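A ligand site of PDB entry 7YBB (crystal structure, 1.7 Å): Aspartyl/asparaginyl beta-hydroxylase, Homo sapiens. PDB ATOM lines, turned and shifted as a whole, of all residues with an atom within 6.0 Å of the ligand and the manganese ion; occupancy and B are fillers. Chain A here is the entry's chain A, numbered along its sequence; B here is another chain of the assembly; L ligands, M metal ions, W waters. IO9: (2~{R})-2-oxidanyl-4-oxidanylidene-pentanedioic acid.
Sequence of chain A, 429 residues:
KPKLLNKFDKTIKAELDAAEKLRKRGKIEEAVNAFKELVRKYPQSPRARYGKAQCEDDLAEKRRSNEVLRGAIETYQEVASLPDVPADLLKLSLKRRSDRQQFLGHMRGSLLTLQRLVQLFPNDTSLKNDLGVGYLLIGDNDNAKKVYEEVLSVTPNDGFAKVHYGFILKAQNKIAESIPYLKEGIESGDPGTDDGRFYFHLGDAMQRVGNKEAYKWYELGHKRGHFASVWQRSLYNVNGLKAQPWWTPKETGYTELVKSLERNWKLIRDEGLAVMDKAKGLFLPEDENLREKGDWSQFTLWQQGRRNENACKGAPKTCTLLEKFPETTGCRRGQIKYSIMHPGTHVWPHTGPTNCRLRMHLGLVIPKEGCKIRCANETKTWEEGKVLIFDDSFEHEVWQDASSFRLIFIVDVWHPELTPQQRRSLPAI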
ATOM      1  N   LEU A 290      -3.363  13.927  30.410  1.00  0.00           N
ATOM      2  CA  LEU A 290      -3.073  13.671  29.008  1.00  0.00           C
ATOM      3  C   LEU A 290      -3.511  12.272  28.557  1.00  0.00           C
ATOM      4  O   LEU A 290      -3.471  11.972  27.359  1.00  0.00           O
ATOM      5  CB  LEU A 290      -1.588  13.868  28.767  1.00  0.00           C
ATOM      6  CG  LEU A 290      -1.007  15.246  29.093  1.00  0.00           C
ATOM      7  CD1 LEU A 290       0.451  15.303  28.868  1.00  0.00           C
ATOM      8  CD2 LEU A 290      -1.714  16.270  28.250  1.00  0.00           C
ATOM      9  N   TRP A 296       0.814   4.924  32.507  1.00  0.00           N
ATOM     10  CA  TRP A 296       1.906   5.767  31.975  1.00  0.00           C
ATOM     11  C   TRP A 296       2.547   6.468  33.155  1.00  0.00           C
ATOM     12  O   TRP A 296       1.885   7.258  33.834  1.00  0.00           O
ATOM     13  CB  TRP A 296       1.343   6.759  30.976  1.00  0.00           C
ATOM     14  CG  TRP A 296       2.267   7.626  30.224  1.00  0.00           C
ATOM     15  CD1 TRP A 296       3.604   7.448  29.974  1.00  0.00           C
ATOM     16  CD2 TRP A 296       1.913   8.879  29.631  1.00  0.00           C
ATOM     17  NE1 TRP A 296       4.072   8.524  29.244  1.00  0.00           N
ATOM     18  CE2 TRP A 296       3.050   9.401  29.025  1.00  0.00           C
ATOM     19  CE3 TRP A 296       0.705   9.592  29.542  1.00  0.00           C
ATOM     20  CZ2 TRP A 296       3.038  10.620  28.334  1.00  0.00           C
ATOM     21  CZ3 TRP A 296       0.700  10.781  28.851  1.00  0.00           C
ATOM     22  CH2 TRP A 296       1.857  11.278  28.253  1.00  0.00           C
ATOM     23  N   GLN A 298       6.445   8.071  34.853  1.00  0.00           N
ATOM     24  CA  GLN A 298       7.774   8.600  34.574  1.00  0.00           C
ATOM     25  C   GLN A 298       8.636   8.668  35.838  1.00  0.00           C
ATOM     26  O   GLN A 298       8.142   9.007  36.907  1.00  0.00           O
ATOM     27  CB  GLN A 298       7.666   9.982  33.929  1.00  0.00           C
ATOM     28  CG  GLN A 298       6.999   9.877  32.610  1.00  0.00           C
ATOM     29  CD  GLN A 298       6.055  10.949  32.424  1.00  0.00           C
ATOM     30  OE1 GLN A 298       6.329  11.916  31.671  1.00  0.00           O
ATOM     31  NE2 GLN A 298       4.914  10.851  33.129  1.00  0.00           N
ATOM     32  N   LYS A 337      14.172  11.882  31.914  1.00  0.00           N
ATOM     33  CA  LYS A 337      13.305  10.944  32.600  1.00  0.00           C
ATOM     34  C   LYS A 337      13.088   9.630  31.866  1.00  0.00           C
ATOM     35  O   LYS A 337      13.042   9.596  30.634  1.00  0.00           O
ATOM     36  CB  LYS A 337      11.940  11.558  32.838  1.00  0.00           C
ATOM     37  CG  LYS A 337      11.202  11.995  31.628  1.00  0.00           C
ATOM     38  CD  LYS A 337       9.993  12.869  32.023  1.00  0.00           C
ATOM     39  CE  LYS A 337       9.393  13.525  30.790  1.00  0.00           C
ATOM     40  NZ  LYS A 337       8.357  14.559  31.049  1.00  0.00           N
ATOM     41  N   SER A 339      10.339   6.807  30.876  1.00  0.00           N
ATOM     42  CA  SER A 339       8.889   6.769  30.711  1.00  0.00           C
ATOM     43  C   SER A 339       8.415   5.365  30.359  1.00  0.00           C
ATOM     44  O   SER A 339       8.891   4.777  29.380  1.00  0.00           O
ATOM     45  CB  SER A 339       8.460   7.760  29.631  1.00  0.00           C
ATOM     46  OG  SER A 339       7.057   7.826  29.479  1.00  0.00           O
ATOM     47  N   ILE A 340       7.509   4.813  31.173  1.00  0.00           N
ATOM     48  CA  ILE A 340       6.989   3.475  30.969  1.00  0.00           C
ATOM     49  C   ILE A 340       5.537   3.625  30.600  1.00  0.00           C
ATOM     50  O   ILE A 340       4.826   4.441  31.197  1.00  0.00           O
ATOM     51  CB  ILE A 340       7.184   2.567  32.199  1.00  0.00           C
ATOM     52  CG1 ILE A 340       6.707   1.163  31.870  1.00  0.00           C
ATOM     53  CG2 ILE A 340       6.541   3.123  33.435  1.00  0.00           C
ATOM     54  CD1 ILE A 340       7.254   0.112  32.765  1.00  0.00           C
ATOM     55  N   MET A 341       5.136   2.925  29.557  1.00  0.00           N
ATOM     56  CA  MET A 341       3.740   2.870  29.128  1.00  0.00           C
ATOM     57  C   MET A 341       3.289   1.425  28.923  1.00  0.00           C
ATOM     58  O   MET A 341       4.003   0.600  28.358  1.00  0.00           O
ATOM     59  CB  MET A 341       3.599   3.697  27.846  1.00  0.00           C
ATOM     60  CG  MET A 341       2.186   3.906  27.444  1.00  0.00           C
ATOM     61  SD  MET A 341       1.974   4.990  26.049  1.00  0.00           S
ATOM     62  CE  MET A 341       2.553   6.512  26.680  1.00  0.00           C
ATOM     63  N   VAL A 347      -2.634   8.148  24.677  1.00  0.00           N
ATOM     64  CA  VAL A 347      -2.359   9.508  25.138  1.00  0.00           C
ATOM     65  C   VAL A 347      -3.022  10.446  24.161  1.00  0.00           C
ATOM     66  O   VAL A 347      -2.748  10.378  22.967  1.00  0.00           O
ATOM     67  CB  VAL A 347      -0.840   9.765  25.187  1.00  0.00           C
ATOM     68  CG1 VAL A 347      -0.502  11.188  25.565  1.00  0.00           C
ATOM     69  CG2 VAL A 347      -0.191   8.762  26.146  1.00  0.00           C
ATOM     70  N   HIS A 350      -1.794  16.189  22.045  1.00  0.00           N
ATOM     71  CA  HIS A 350      -1.454  17.300  22.920  1.00  0.00           C
ATOM     72  C   HIS A 350      -0.173  17.933  22.410  1.00  0.00           C
ATOM     73  O   HIS A 350       0.477  17.421  21.498  1.00  0.00           O
ATOM     74  CB  HIS A 350      -1.268  16.861  24.374  1.00  0.00           C
ATOM     75  CG  HIS A 350      -0.033  16.045  24.583  1.00  0.00           C
ATOM     76  ND1 HIS A 350       0.045  14.713  24.226  1.00  0.00           N
ATOM     77  CD2 HIS A 350       1.164  16.375  25.115  1.00  0.00           C
ATOM     78  CE1 HIS A 350       1.250  14.255  24.541  1.00  0.00           C
ATOM     79  NE2 HIS A 350       1.953  15.257  25.073  1.00  0.00           N
ATOM     80  N   THR A 351       0.183  19.040  23.044  1.00  0.00           N
ATOM     81  CA  THR A 351       1.286  19.914  22.698  1.00  0.00           C
ATOM     82  C   THR A 351       1.989  20.283  23.982  1.00  0.00           C
ATOM     83  O   THR A 351       1.328  20.518  24.985  1.00  0.00           O
ATOM     84  CB  THR A 351       0.744  21.168  21.990  1.00  0.00           C
ATOM     85  OG1 THR A 351       0.372  20.835  20.646  1.00  0.00           O
ATOM     86  CG2 THR A 351       1.681  22.222  22.056  1.00  0.00           C
ATOM     87  N   GLY A 352       3.318  20.297  23.991  1.00  0.00           N
ATOM     88  CA  GLY A 352       4.029  20.808  25.126  1.00  0.00           C
ATOM     89  C   GLY A 352       3.968  22.340  25.196  1.00  0.00           C
ATOM     90  O   GLY A 352       3.515  23.011  24.260  1.00  0.00           O
ATOM     91  N   ARG A 359      12.749  17.179  21.884  1.00  0.00           N
ATOM     92  CA  ARG A 359      12.638  15.966  22.716  1.00  0.00           C
ATOM     93  C   ARG A 359      13.293  14.764  22.059  1.00  0.00           C
ATOM     94  O   ARG A 359      12.888  14.329  20.963  1.00  0.00           O
ATOM     95  CB  ARG A 359      11.156  15.699  23.008  1.00  0.00           C
ATOM     96  CG  ARG A 359      10.789  14.637  24.032  1.00  0.00           C
ATOM     97  CD  ARG A 359       9.593  15.075  24.851  1.00  0.00           C
ATOM     98  NE  ARG A 359       9.918  15.905  26.002  1.00  0.00           N
ATOM     99  CZ  ARG A 359       9.077  16.056  27.027  1.00  0.00           C
ATOM    100  NH1 ARG A 359       7.922  15.474  26.961  1.00  0.00           N
ATOM    101  NH2 ARG A 359       9.370  16.801  28.072  1.00  0.00           N
ATOM    102  N   HIS A 361      14.007  10.673  22.302  1.00  0.00           N
ATOM    103  CA  HIS A 361      13.535   9.415  22.885  1.00  0.00           C
ATOM    104  C   HIS A 361      14.527   8.315  22.532  1.00  0.00           C
ATOM    105  O   HIS A 361      14.762   8.043  21.345  1.00  0.00           O
ATOM    106  CB  HIS A 361      12.152   8.969  22.371  1.00  0.00           C
ATOM    107  CG  HIS A 361      10.972   9.730  22.888  1.00  0.00           C
ATOM    108  ND1 HIS A 361       9.689   9.326  22.600  1.00  0.00           N
ATOM    109  CD2 HIS A 361      10.856  10.801  23.697  1.00  0.00           C
ATOM    110  CE1 HIS A 361       8.834  10.118  23.208  1.00  0.00           C
ATOM    111  NE2 HIS A 361       9.515  11.057  23.842  1.00  0.00           N
ATOM    112  N   ILE A 373       4.037   6.502  17.833  1.00  0.00           N
ATOM    113  CA  ILE A 373       3.956   7.906  18.225  1.00  0.00           C
ATOM    114  C   ILE A 373       3.774   8.744  16.957  1.00  0.00           C
ATOM    115  O   ILE A 373       4.609   8.679  16.051  1.00  0.00           O
ATOM    116  CB  ILE A 373       5.193   8.388  19.002  1.00  0.00           C
ATOM    117  CG1 ILE A 373       5.150   9.888  19.209  1.00  0.00           C
ATOM    118  CG2 ILE A 373       6.486   8.038  18.287  1.00  0.00           C
ATOM    119  CD1 ILE A 373       5.993  10.430  20.335  1.00  0.00           C
ATOM    120  N   TRP A 382       9.412   3.336  17.793  1.00  0.00           N
ATOM    121  CA  TRP A 382      10.736   3.319  18.417  1.00  0.00           C
ATOM    122  C   TRP A 382      11.508   2.062  18.056  1.00  0.00           C
ATOM    123  O   TRP A 382      10.959   1.078  17.563  1.00  0.00           O
ATOM    124  CB  TRP A 382      10.602   3.421  19.931  1.00  0.00           C
ATOM    125  CG  TRP A 382       9.854   4.607  20.453  1.00  0.00           C
ATOM    126  CD1 TRP A 382      10.393   5.778  20.778  1.00  0.00           C
ATOM    127  CD2 TRP A 382       8.447   4.729  20.745  1.00  0.00           C
ATOM    128  NE1 TRP A 382       9.463   6.639  21.234  1.00  0.00           N
ATOM    129  CE2 TRP A 382       8.253   6.017  21.257  1.00  0.00           C
ATOM    130  CE3 TRP A 382       7.351   3.892  20.625  1.00  0.00           C
ATOM    131  CZ2 TRP A 382       6.997   6.497  21.611  1.00  0.00           C
ATOM    132  CZ3 TRP A 382       6.111   4.376  20.994  1.00  0.00           C
ATOM    133  CH2 TRP A 382       5.945   5.651  21.486  1.00  0.00           C
ATOM    134  N   PHE A 390      11.865  14.663  18.177  1.00  0.00           N
ATOM    135  CA  PHE A 390      10.722  15.418  17.664  1.00  0.00           C
ATOM    136  C   PHE A 390      10.601  16.713  18.448  1.00  0.00           C
ATOM    137  O   PHE A 390      11.140  16.851  19.542  1.00  0.00           O
ATOM    138  CB  PHE A 390       9.443  14.573  17.686  1.00  0.00           C
ATOM    139  CG  PHE A 390       8.927  14.217  19.051  1.00  0.00           C
ATOM    140  CD1 PHE A 390       9.502  13.209  19.791  1.00  0.00           C
ATOM    141  CD2 PHE A 390       7.808  14.817  19.544  1.00  0.00           C
ATOM    142  CE1 PHE A 390       8.996  12.881  21.000  1.00  0.00           C
ATOM    143  CE2 PHE A 390       7.293  14.466  20.717  1.00  0.00           C
ATOM    144  CZ  PHE A 390       7.873  13.530  21.457  1.00  0.00           C
ATOM    145  N   ASP A 392       8.142  18.596  20.479  1.00  0.00           N
ATOM    146  CA  ASP A 392       6.880  18.293  21.146  1.00  0.00           C
ATOM    147  C   ASP A 392       6.010  19.539  21.308  1.00  0.00           C
ATOM    148  O   ASP A 392       4.914  19.437  21.868  1.00  0.00           O
ATOM    149  CB  ASP A 392       7.159  17.583  22.481  1.00  0.00           C
ATOM    150  CG  ASP A 392       7.423  18.522  23.651  1.00  0.00           C
ATOM    151  OD1 ASP A 392       8.133  19.534  23.505  1.00  0.00           O
ATOM    152  OD2 ASP A 392       6.858  18.186  24.733  1.00  0.00           O
ATOM    153  N   HIS A 396       1.053  15.935  19.181  1.00  0.00           N
ATOM    154  CA  HIS A 396       1.532  14.566  19.100  1.00  0.00           C
ATOM    155  C   HIS A 396       0.670  13.666  19.962  1.00  0.00           C
ATOM    156  O   HIS A 396      -0.061  14.106  20.848  1.00  0.00           O
ATOM    157  CB  HIS A 396       3.030  14.458  19.469  1.00  0.00           C
ATOM    158  CG  HIS A 396       3.370  15.020  20.808  1.00  0.00           C
ATOM    159  ND1 HIS A 396       3.501  16.367  21.034  1.00  0.00           N
ATOM    160  CD2 HIS A 396       3.560  14.408  22.003  1.00  0.00           C
ATOM    161  CE1 HIS A 396       3.763  16.578  22.305  1.00  0.00           C
ATOM    162  NE2 HIS A 396       3.812  15.407  22.924  1.00  0.00           N
ATOM    163  N   VAL A 398       0.159   9.252  21.236  1.00  0.00           N
ATOM    164  CA  VAL A 398       0.825   7.970  21.484  1.00  0.00           C
ATOM    165  C   VAL A 398      -0.184   6.871  21.771  1.00  0.00           C
ATOM    166  O   VAL A 398      -1.194   7.093  22.464  1.00  0.00           O
ATOM    167  CB  VAL A 398       1.821   8.098  22.649  1.00  0.00           C
ATOM    168  CG1 VAL A 398       2.632   6.919  22.768  1.00  0.00           C
ATOM    169  CG2 VAL A 398       2.703   9.285  22.483  1.00  0.00           C
ATOM    170  N   ARG A 406       6.428  -1.063  27.576  1.00  0.00           N
ATOM    171  CA  ARG A 406       7.317  -0.290  26.709  1.00  0.00           C
ATOM    172  C   ARG A 406       8.050   0.750  27.536  1.00  0.00           C
ATOM    173  O   ARG A 406       7.434   1.621  28.155  1.00  0.00           O
ATOM    174  CB  ARG A 406       6.520   0.374  25.621  1.00  0.00           C
ATOM    175  CG  ARG A 406       7.319   1.184  24.685  1.00  0.00           C
ATOM    176  CD  ARG A 406       6.740   2.531  24.526  1.00  0.00           C
ATOM    177  NE  ARG A 406       6.922   3.308  25.757  1.00  0.00           N
ATOM    178  CZ  ARG A 406       6.605   4.585  25.918  1.00  0.00           C
ATOM    179  NH1 ARG A 406       6.042   5.301  24.953  1.00  0.00           N
ATOM    180  NH2 ARG A 406       6.848   5.189  27.062  1.00  0.00           N
ATOM    181  N   ILE A 408      11.019   3.737  27.558  1.00  0.00           N
ATOM    182  CA  ILE A 408      11.888   4.664  26.840  1.00  0.00           C
ATOM    183  C   ILE A 408      12.616   5.595  27.789  1.00  0.00           C
ATOM    184  O   ILE A 408      12.185   5.807  28.916  1.00  0.00           O
ATOM    185  CB  ILE A 408      11.122   5.512  25.772  1.00  0.00           C
ATOM    186  CG1 ILE A 408      10.093   6.488  26.379  1.00  0.00           C
ATOM    187  CG2 ILE A 408      10.494   4.611  24.675  1.00  0.00           C
ATOM    188  CD1 ILE A 408       9.533   7.436  25.277  1.00  0.00           C
ATOM    189  N   ILE A 410      13.822   9.612  28.004  1.00  0.00           N
ATOM    190  CA  ILE A 410      13.472  10.917  27.424  1.00  0.00           C
ATOM    191  C   ILE A 410      14.513  11.946  27.852  1.00  0.00           C
ATOM    192  O   ILE A 410      14.756  12.130  29.059  1.00  0.00           O
ATOM    193  CB  ILE A 410      12.069  11.394  27.821  1.00  0.00           C
ATOM    194  CG1 ILE A 410      11.037  10.377  27.421  1.00  0.00           C
ATOM    195  CG2 ILE A 410      11.709  12.650  27.102  1.00  0.00           C
ATOM    196  CD1 ILE A 410       9.606  10.768  27.614  1.00  0.00           C
ATOM    197  N   ASP B  18       4.848  17.985  30.284  1.00  0.00           N
ATOM    198  CA  ASP B  18       4.537  17.604  28.902  1.00  0.00           C
ATOM    199  C   ASP B  18       3.410  18.451  28.285  1.00  0.00           C
ATOM    200  O   ASP B  18       3.198  18.409  27.072  1.00  0.00           O
ATOM    201  CB  ASP B  18       4.135  16.124  28.833  1.00  0.00           C
ATOM    202  CG  ASP B  18       5.318  15.159  28.962  1.00  0.00           C
ATOM    203  OD1 ASP B  18       6.432  15.605  29.263  1.00  0.00           O
ATOM    204  OD2 ASP B  18       5.142  13.946  28.757  1.00  0.00           O
HETATM  205  C01 IO9 L   1       6.108   8.505  26.045  1.00  0.00           C
HETATM  206  C02 IO9 L   1       6.103  12.976  24.973  1.00  0.00           C
HETATM  207  C03 IO9 L   1       6.050  10.028  26.114  1.00  0.00           C
HETATM  208  C04 IO9 L   1       5.081  10.601  25.068  1.00  0.00           C
HETATM  209  C05 IO9 L   1       5.021  12.171  25.046  1.00  0.00           C
HETATM  210  O01 IO9 L   1       5.862   7.981  24.828  1.00  0.00           O
HETATM  211  O02 IO9 L   1       6.290   7.781  27.042  1.00  0.00           O
HETATM  212  O03 IO9 L   1       7.428  12.435  25.040  1.00  0.00           O
HETATM  213  O04 IO9 L   1       6.150  14.169  24.894  1.00  0.00           O
HETATM  214  O05 IO9 L   1       5.850  10.437  27.443  1.00  0.00           O
HETATM  215  O06 IO9 L   1       3.921  12.710  25.133  1.00  0.00           O
HETATM  216 MN    MN M   1       4.132  14.837  25.009  1.00  0.00          MN
HETATM  217  O   HOH W   1       4.630  16.697  25.574  1.00  0.00           O
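Residues that only touch the manganese ion: Asp 18 of chain B.
Within 4 Å of the manganese ion: His 350, His 396 and Asp 18 of chain B.
Along chain A the residues within 4 Å of the manganese ion span positions 350 to 396.
Water W1 binds the manganese ion (2.0 Å).
The manganese ion is bound by O04 of the ligand (2.1 Å).
The manganese ion is bound by an oxygen (O06) of the ligand.
The manganese ion is bound by NE2 of His 396 (2.2 Å).
NE2 of His 350 binds the manganese ion.
The manganese ion has five donor atoms within binding distance.
Water W1 lies within hydrogen-bond range of the backbone carbonyl oxygen (O) of Asp 18 of chain B (2.7 Å) and the side-chain carboxylate (OD2) of Asp 392 (2.8 Å).
A ring nitrogen (ND1) of His 361 sits at hydrogen-bond distance from the indole nitrogen of Trp 382, at 3.0 Å.
The backbone carbonyl oxygen (O) of Asp 392 sits close to a ring nitrogen (ND1) of His 396, 3.5 Å away.
The backbone NH (N) of Ile 410 is in hydrogen-bond range of the backbone carbonyl oxygen (O) of Lys 337.
OG of Ser 339 lies within hydrogen-bond range of NE1 of Trp 296 (3.1 Å).
The backbone carbonyl oxygen (O) of Arg 406 is in hydrogen-bond range of the backbone NH (N) of Met 341 (3.0 Å).
O of Ser 339 lies within hydrogen-bond range of NH2 of Arg 406 (3.1 Å).
N of Val 347 sits at hydrogen-bond distance from O of Val 398.
The backbone NH of Ser 339 lies within hydrogen-bond range of the backbone carbonyl oxygen of Ile 408.
The guanidinium group (NH2) of Arg 406 lies within salt-bridge range of an oxygen (O02) of the ligand (2.7 Å).
A ring nitrogen (NE2) of His 361 sits at hydrogen-bond distance from an oxygen (O03) of the ligand, 2.8 Å away.
The side-chain hydroxyl of Ser 339 lies within hydrogen-bond range of an oxygen (O02) of the ligand (2.6 Å).
O03 of the ligand lies within salt-bridge range of NH1 of Arg 359 (3.6 Å).
O05 of the ligand lies close to NE1 of Trp 296 (3.2 Å).
CE of Met 341 touches O02 of the ligand, 3.96 Å away.
Trp 382 touches the ligand (CZ2 to O01, 3.7 Å).
Phe 390 touches the ligand.
CG2 of Val 398 touches C04 of the ligand, at 3.8 Å.
CD1 of Ile 408 touches C01 of the ligand (3.7 Å).
Ile 410 touches the ligand (CD1 to O03, 3.8 Å).
OD2 of Asp 18 of chain B touches O05 of the ligand, 3.8 Å away.
The nearest printed residue that does not touch the ligand is Asp 392 (4.1 Å).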
